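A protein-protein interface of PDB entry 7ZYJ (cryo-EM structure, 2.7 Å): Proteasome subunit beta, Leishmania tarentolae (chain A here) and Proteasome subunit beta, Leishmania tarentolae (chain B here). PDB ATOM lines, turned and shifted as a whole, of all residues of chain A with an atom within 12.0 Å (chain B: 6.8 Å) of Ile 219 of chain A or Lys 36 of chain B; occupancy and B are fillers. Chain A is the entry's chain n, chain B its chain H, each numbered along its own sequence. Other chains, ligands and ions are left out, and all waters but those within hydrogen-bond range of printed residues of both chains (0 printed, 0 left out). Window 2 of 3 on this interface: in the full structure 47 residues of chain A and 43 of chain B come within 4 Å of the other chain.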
ATOM      1  N   CYS A 212      -6.529 -11.062 -24.380  1.00  0.00           N
ATOM      2  CA  CYS A 212      -7.141 -11.759 -23.261  1.00  0.00           C
ATOM      3  C   CYS A 212      -6.155 -12.732 -22.617  1.00  0.00           C
ATOM      4  O   CYS A 212      -5.083 -13.031 -23.150  1.00  0.00           O
ATOM      5  CB  CYS A 212      -8.400 -12.498 -23.713  1.00  0.00           C
ATOM      6  SG  CYS A 212      -8.150 -13.632 -25.090  1.00  0.00           S
ATOM      7  N   PHE A 213      -6.542 -13.224 -21.437  1.00  0.00           N
ATOM      8  CA  PHE A 213      -5.671 -14.102 -20.662  1.00  0.00           C
ATOM      9  C   PHE A 213      -5.390 -15.414 -21.383  1.00  0.00           C
ATOM     10  O   PHE A 213      -4.256 -15.903 -21.356  1.00  0.00           O
ATOM     11  CB  PHE A 213      -6.301 -14.367 -19.295  1.00  0.00           C
ATOM     12  CG  PHE A 213      -5.339 -14.895 -18.268  1.00  0.00           C
ATOM     13  CD1 PHE A 213      -5.001 -16.237 -18.237  1.00  0.00           C
ATOM     14  CD2 PHE A 213      -4.780 -14.048 -17.328  1.00  0.00           C
ATOM     15  CE1 PHE A 213      -4.121 -16.722 -17.291  1.00  0.00           C
ATOM     16  CE2 PHE A 213      -3.899 -14.528 -16.379  1.00  0.00           C
ATOM     17  CZ  PHE A 213      -3.568 -15.866 -16.361  1.00  0.00           C
ATOM     18  N   GLU A 214      -6.400 -16.001 -22.030  1.00  0.00           N
ATOM     19  CA  GLU A 214      -6.224 -17.326 -22.613  1.00  0.00           C
ATOM     20  C   GLU A 214      -5.467 -17.292 -23.935  1.00  0.00           C
ATOM     21  O   GLU A 214      -4.723 -18.232 -24.237  1.00  0.00           O
ATOM     22  CB  GLU A 214      -7.582 -18.012 -22.790  1.00  0.00           C
ATOM     23  CG  GLU A 214      -8.489 -17.406 -23.849  1.00  0.00           C
ATOM     24  CD  GLU A 214      -9.307 -16.237 -23.327  1.00  0.00           C
ATOM     25  OE1 GLU A 214      -8.970 -15.700 -22.250  1.00  0.00           O
ATOM     26  OE2 GLU A 214     -10.292 -15.857 -23.994  1.00  0.00           O
ATOM     27  N   LYS A 215      -5.630 -16.236 -24.734  1.00  0.00           N
ATOM     28  CA  LYS A 215      -4.915 -16.167 -26.004  1.00  0.00           C
ATOM     29  C   LYS A 215      -3.447 -15.809 -25.818  1.00  0.00           C
ATOM     30  O   LYS A 215      -2.604 -16.239 -26.613  1.00  0.00           O
ATOM     31  CB  LYS A 215      -5.584 -15.160 -26.940  1.00  0.00           C
ATOM     32  CG  LYS A 215      -6.612 -15.772 -27.874  1.00  0.00           C
ATOM     33  CD  LYS A 215      -7.171 -14.733 -28.831  1.00  0.00           C
ATOM     34  CE  LYS A 215      -8.431 -15.233 -29.517  1.00  0.00           C
ATOM     35  NZ  LYS A 215      -8.144 -16.334 -30.478  1.00  0.00           N
ATOM     36  N   THR A 216      -3.122 -15.033 -24.789  1.00  0.00           N
ATOM     37  CA  THR A 216      -1.746 -14.648 -24.512  1.00  0.00           C
ATOM     38  C   THR A 216      -1.040 -15.614 -23.572  1.00  0.00           C
ATOM     39  O   THR A 216       0.152 -15.433 -23.303  1.00  0.00           O
ATOM     40  CB  THR A 216      -1.700 -13.237 -23.918  1.00  0.00           C
ATOM     41  OG1 THR A 216      -2.617 -13.149 -22.822  1.00  0.00           O
ATOM     42  CG2 THR A 216      -2.075 -12.204 -24.967  1.00  0.00           C
ATOM     43  N   ALA A 217      -1.737 -16.630 -23.073  1.00  0.00           N
ATOM     44  CA  ALA A 217      -1.137 -17.556 -22.125  1.00  0.00           C
ATOM     45  C   ALA A 217      -0.141 -18.475 -22.817  1.00  0.00           C
ATOM     46  O   ALA A 217      -0.318 -18.855 -23.978  1.00  0.00           O
ATOM     47  CB  ALA A 217      -2.218 -18.385 -21.435  1.00  0.00           C
ATOM     48  N   ILE A 218       0.918 -18.829 -22.092  1.00  0.00           N
ATOM     49  CA  ILE A 218       1.896 -19.801 -22.564  1.00  0.00           C
ATOM     50  C   ILE A 218       1.729 -21.073 -21.744  1.00  0.00           C
ATOM     51  O   ILE A 218       2.329 -21.216 -20.673  1.00  0.00           O
ATOM     52  CB  ILE A 218       3.327 -19.246 -22.450  1.00  0.00           C
ATOM     53  CG1 ILE A 218       3.419 -17.877 -23.124  1.00  0.00           C
ATOM     54  CG2 ILE A 218       4.327 -20.214 -23.060  1.00  0.00           C
ATOM     55  CD1 ILE A 218       4.661 -17.102 -22.762  1.00  0.00           C
ATOM     56  N   ILE A 219       0.918 -22.002 -22.234  1.00  0.00           N
ATOM     57  CA  ILE A 219       0.612 -23.207 -21.473  1.00  0.00           C
ATOM     58  C   ILE A 219       1.714 -24.243 -21.645  1.00  0.00           C
ATOM     59  O   ILE A 219       2.661 -24.285 -20.861  1.00  0.00           O
ATOM     60  CB  ILE A 219      -0.756 -23.786 -21.874  1.00  0.00           C
ATOM     61  CG1 ILE A 219      -0.889 -23.846 -23.396  1.00  0.00           C
ATOM     62  CG2 ILE A 219      -1.879 -22.962 -21.268  1.00  0.00           C
ATOM     63  CD1 ILE A 219      -2.184 -24.467 -23.872  1.00  0.00           C
ATOM     64  N   LEU B  34       1.864 -14.934 -15.999  1.00  0.00           N
ATOM     65  CA  LEU B  34       1.322 -15.996 -15.156  1.00  0.00           C
ATOM     66  C   LEU B  34       1.224 -17.247 -16.021  1.00  0.00           C
ATOM     67  O   LEU B  34       0.317 -17.375 -16.846  1.00  0.00           O
ATOM     68  CB  LEU B  34      -0.030 -15.596 -14.575  1.00  0.00           C
ATOM     69  CG  LEU B  34      -0.086 -14.231 -13.887  1.00  0.00           C
ATOM     70  CD1 LEU B  34      -1.502 -13.912 -13.439  1.00  0.00           C
ATOM     71  CD2 LEU B  34       0.876 -14.179 -12.713  1.00  0.00           C
ATOM     72  N   THR B  35       2.163 -18.168 -15.831  1.00  0.00           N
ATOM     73  CA  THR B  35       2.317 -19.333 -16.687  1.00  0.00           C
ATOM     74  C   THR B  35       1.788 -20.568 -15.975  1.00  0.00           C
ATOM     75  O   THR B  35       2.175 -20.850 -14.835  1.00  0.00           O
ATOM     76  CB  THR B  35       3.783 -19.531 -17.075  1.00  0.00           C
ATOM     77  OG1 THR B  35       4.260 -18.363 -17.755  1.00  0.00           O
ATOM     78  CG2 THR B  35       3.936 -20.735 -17.982  1.00  0.00           C
ATOM     79  N   LYS B  36       0.899 -21.290 -16.651  1.00  0.00           N
ATOM     80  CA  LYS B  36       0.298 -22.491 -16.090  1.00  0.00           C
ATOM     81  C   LYS B  36       1.313 -23.624 -16.022  1.00  0.00           C
ATOM     82  O   LYS B  36       1.983 -23.935 -17.011  1.00  0.00           O
ATOM     83  CB  LYS B  36      -0.899 -22.911 -16.940  1.00  0.00           C
ATOM     84  CG  LYS B  36      -1.666 -24.098 -16.404  1.00  0.00           C
ATOM     85  CD  LYS B  36      -2.876 -24.392 -17.269  1.00  0.00           C
ATOM     86  CE  LYS B  36      -3.650 -25.588 -16.749  1.00  0.00           C
ATOM     87  NZ  LYS B  36      -4.837 -25.882 -17.598  1.00  0.00           N
ATOM     88  N   LEU B  37       1.427 -24.243 -14.847  1.00  0.00           N
ATOM     89  CA  LEU B  37       2.218 -25.457 -14.677  1.00  0.00           C
ATOM     90  C   LEU B  37       1.324 -26.691 -14.653  1.00  0.00           C
ATOM     91  O   LEU B  37       1.452 -27.582 -15.498  1.00  0.00           O
ATOM     92  CB  LEU B  37       3.031 -25.368 -13.383  1.00  0.00           C
ATOM     93  CG  LEU B  37       3.886 -24.114 -13.223  1.00  0.00           C
ATOM     94  CD1 LEU B  37       4.566 -24.129 -11.873  1.00  0.00           C
ATOM     95  CD2 LEU B  37       4.902 -24.011 -14.347  1.00  0.00           C
ATOM     96  N   THR B  38       0.412 -26.751 -13.692  1.00  0.00           N
ATOM     97  CA  THR B  38      -0.684 -27.707 -13.642  1.00  0.00           C
ATOM     98  C   THR B  38      -1.989 -26.918 -13.579  1.00  0.00           C
ATOM     99  O   THR B  38      -2.004 -25.695 -13.737  1.00  0.00           O
ATOM    100  CB  THR B  38      -0.537 -28.664 -12.456  1.00  0.00           C
ATOM    101  OG1 THR B  38      -0.776 -27.958 -11.233  1.00  0.00           O
ATOM    102  CG2 THR B  38       0.856 -29.275 -12.424  1.00  0.00           C
ATOM    103  N   LYS B  39      -3.094 -27.625 -13.343  1.00  0.00           N
ATOM    104  CA  LYS B  39      -4.389 -26.957 -13.283  1.00  0.00           C
ATOM    105  C   LYS B  39      -4.441 -25.947 -12.142  1.00  0.00           C
ATOM    106  O   LYS B  39      -4.989 -24.850 -12.301  1.00  0.00           O
ATOM    107  CB  LYS B  39      -5.508 -27.987 -13.138  1.00  0.00           C
ATOM    108  CG  LYS B  39      -6.882 -27.449 -13.496  1.00  0.00           C
ATOM    109  CD  LYS B  39      -7.961 -28.063 -12.624  1.00  0.00           C
ATOM    110  CE  LYS B  39      -9.334 -27.527 -12.994  1.00  0.00           C
ATOM    111  NZ  LYS B  39     -10.412 -28.510 -12.696  1.00  0.00           N
ATOM    112  N   LYS B  40      -3.877 -26.294 -10.986  1.00  0.00           N
ATOM    113  CA  LYS B  40      -3.971 -25.460  -9.795  1.00  0.00           C
ATOM    114  C   LYS B  40      -2.640 -24.841  -9.379  1.00  0.00           C
ATOM    115  O   LYS B  40      -2.566 -24.239  -8.306  1.00  0.00           O
ATOM    116  CB  LYS B  40      -4.547 -26.266  -8.631  1.00  0.00           C
ATOM    117  CG  LYS B  40      -5.962 -26.761  -8.855  1.00  0.00           C
ATOM    118  CD  LYS B  40      -6.921 -25.605  -9.070  1.00  0.00           C
ATOM    119  CE  LYS B  40      -8.353 -26.095  -9.173  1.00  0.00           C
ATOM    120  NZ  LYS B  40      -8.778 -26.829  -7.951  1.00  0.00           N
ATOM    121  N   ILE B  41      -1.592 -24.969 -10.189  1.00  0.00           N
ATOM    122  CA  ILE B  41      -0.278 -24.426  -9.860  1.00  0.00           C
ATOM    123  C   ILE B  41       0.192 -23.552 -11.013  1.00  0.00           C
ATOM    124  O   ILE B  41       0.170 -23.983 -12.171  1.00  0.00           O
ATOM    125  CB  ILE B  41       0.751 -25.537  -9.570  1.00  0.00           C
ATOM    126  CG1 ILE B  41       0.234 -26.476  -8.481  1.00  0.00           C
ATOM    127  CG2 ILE B  41       2.081 -24.933  -9.156  1.00  0.00           C
ATOM    128  CD1 ILE B  41       1.085 -27.707  -8.285  1.00  0.00           C
ATOM    129  N   TYR B  42       0.619 -22.330 -10.698  1.00  0.00           N
ATOM    130  CA  TYR B  42       1.100 -21.378 -11.686  1.00  0.00           C
ATOM    131  C   TYR B  42       2.432 -20.801 -11.226  1.00  0.00           C
ATOM    132  O   TYR B  42       2.840 -20.953 -10.069  1.00  0.00           O
ATOM    133  CB  TYR B  42       0.088 -20.247 -11.921  1.00  0.00           C
ATOM    134  CG  TYR B  42      -1.000 -20.573 -12.918  1.00  0.00           C
ATOM    135  CD1 TYR B  42      -1.881 -21.622 -12.697  1.00  0.00           C
ATOM    136  CD2 TYR B  42      -1.148 -19.827 -14.077  1.00  0.00           C
ATOM    137  CE1 TYR B  42      -2.873 -21.923 -13.604  1.00  0.00           C
ATOM    138  CE2 TYR B  42      -2.140 -20.118 -14.990  1.00  0.00           C
ATOM    139  CZ  TYR B  42      -2.999 -21.167 -14.749  1.00  0.00           C
ATOM    140  OH  TYR B  42      -3.990 -21.462 -15.657  1.00  0.00           O
ATOM    141  N   CYS B  43       3.115 -20.138 -12.157  1.00  0.00           N
ATOM    142  CA  CYS B  43       4.364 -19.455 -11.850  1.00  0.00           C
ATOM    143  C   CYS B  43       4.353 -18.047 -12.428  1.00  0.00           C
ATOM    144  O   CYS B  43       3.865 -17.817 -13.537  1.00  0.00           O
ATOM    145  CB  CYS B  43       5.579 -20.232 -12.381  1.00  0.00           C
ATOM    146  SG  CYS B  43       5.690 -20.361 -14.175  1.00  0.00           S
ATOM    147  N   ALA B  56       9.641 -22.840 -17.615  1.00  0.00           N
ATOM    148  CA  ALA B  56       8.255 -23.160 -17.303  1.00  0.00           C
ATOM    149  C   ALA B  56       7.739 -24.300 -18.167  1.00  0.00           C
ATOM    150  O   ALA B  56       7.040 -25.188 -17.671  1.00  0.00           O
ATOM    151  CB  ALA B  56       7.380 -21.919 -17.472  1.00  0.00           C
ATOM    152  N   GLU B  57       8.067 -24.295 -19.461  1.00  0.00           N
ATOM    153  CA  GLU B  57       7.620 -25.376 -20.334  1.00  0.00           C
ATOM    154  C   GLU B  57       8.222 -26.712 -19.915  1.00  0.00           C
ATOM    155  O   GLU B  57       7.520 -27.730 -19.875  1.00  0.00           O
ATOM    156  CB  GLU B  57       7.964 -25.052 -21.787  1.00  0.00           C
ATOM    157  CG  GLU B  57       7.184 -23.871 -22.345  1.00  0.00           C
ATOM    158  CD  GLU B  57       7.550 -23.546 -23.778  1.00  0.00           C
ATOM    159  OE1 GLU B  57       8.502 -24.157 -24.305  1.00  0.00           O
ATOM    160  OE2 GLU B  57       6.883 -22.679 -24.380  1.00  0.00           O
ATOM    161  N   SER B  60       6.515 -27.820 -16.653  1.00  0.00           N
ATOM    162  CA  SER B  60       5.151 -28.263 -16.915  1.00  0.00           C
ATOM    163  C   SER B  60       5.135 -29.632 -17.581  1.00  0.00           C
ATOM    164  O   SER B  60       4.295 -30.478 -17.252  1.00  0.00           O
ATOM    165  CB  SER B  60       4.424 -27.234 -17.780  1.00  0.00           C
ATOM    166  OG  SER B  60       3.084 -27.619 -18.017  1.00  0.00           O
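O of Cys 43 of chain B sits at hydrogen-bond distance from N of Thr 35 of chain B (2.9 Å).
CD1 of Leu 34 of chain B touches CE2 of Phe 213 of chain A, at 3.8 Å.
Ile 218 of chain A touches Thr 35 of chain B.
Ile 218 of chain A touches Glu 57 of chain B.
Ile 219 of chain A touches Lys 36 of chain B.
Ile 219 of chain A touches just one residue of chain B: Lys 36 (3.9 Å).
Thr 35 of chain B touches just one residue of chain A: Ile 218.
No residue of chain A comes within 4 Å of Thr 38 of chain B.
No residue of chain A comes within 4 Å of Lys 39 of chain B.
No residue of chain A comes within 4 Å of Cys 43 of chain B.
No residue of chain A comes within 4 Å of Ala 56 of chain B.
Of chain A, only Ile 218 (3.8 Å) comes within 4 Å of Glu 57 of chain B.
Ser 60 of chain B touches none of the printed residues of chain A.
Printed residues of chain B within 4 Å of Ile 218 of chain A: Thr 35 (3.2 Å) and Glu 57 (3.8 Å).
Of the printed residues of chain A, Leu 34 of chain B touches Phe 213 (3.8 Å).
Of the printed residues of chain B, Phe 213 of chain A touches Leu 34 (3.8 Å).
Glu 214 of chain A touches none of the printed residues of chain B.
Thr 216 of chain A touches none of the printed residues of chain B.
The nearest printed residue of chain B that does not touch Ile 218 of chain A is Lys 36 of chain B (4.3 Å).
Printed residues of chain B that touch a printed residue of chain A: Leu 34, Thr 35, Lys 36 and Glu 57.
Hydrophobic or aromatic side chains of chain B within 4 Å of the printed part of chain A: Leu 34.
Of the 8 printed residues of chain A, 3 touch a printed residue of chain B.
Hydrophobic or aromatic side chains of chain A within 4 Å of the printed part of chain B: Phe 213 and Ile 218.
Along chain A the printed residues that touch a printed residue of chain B span positions 213 to 219.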
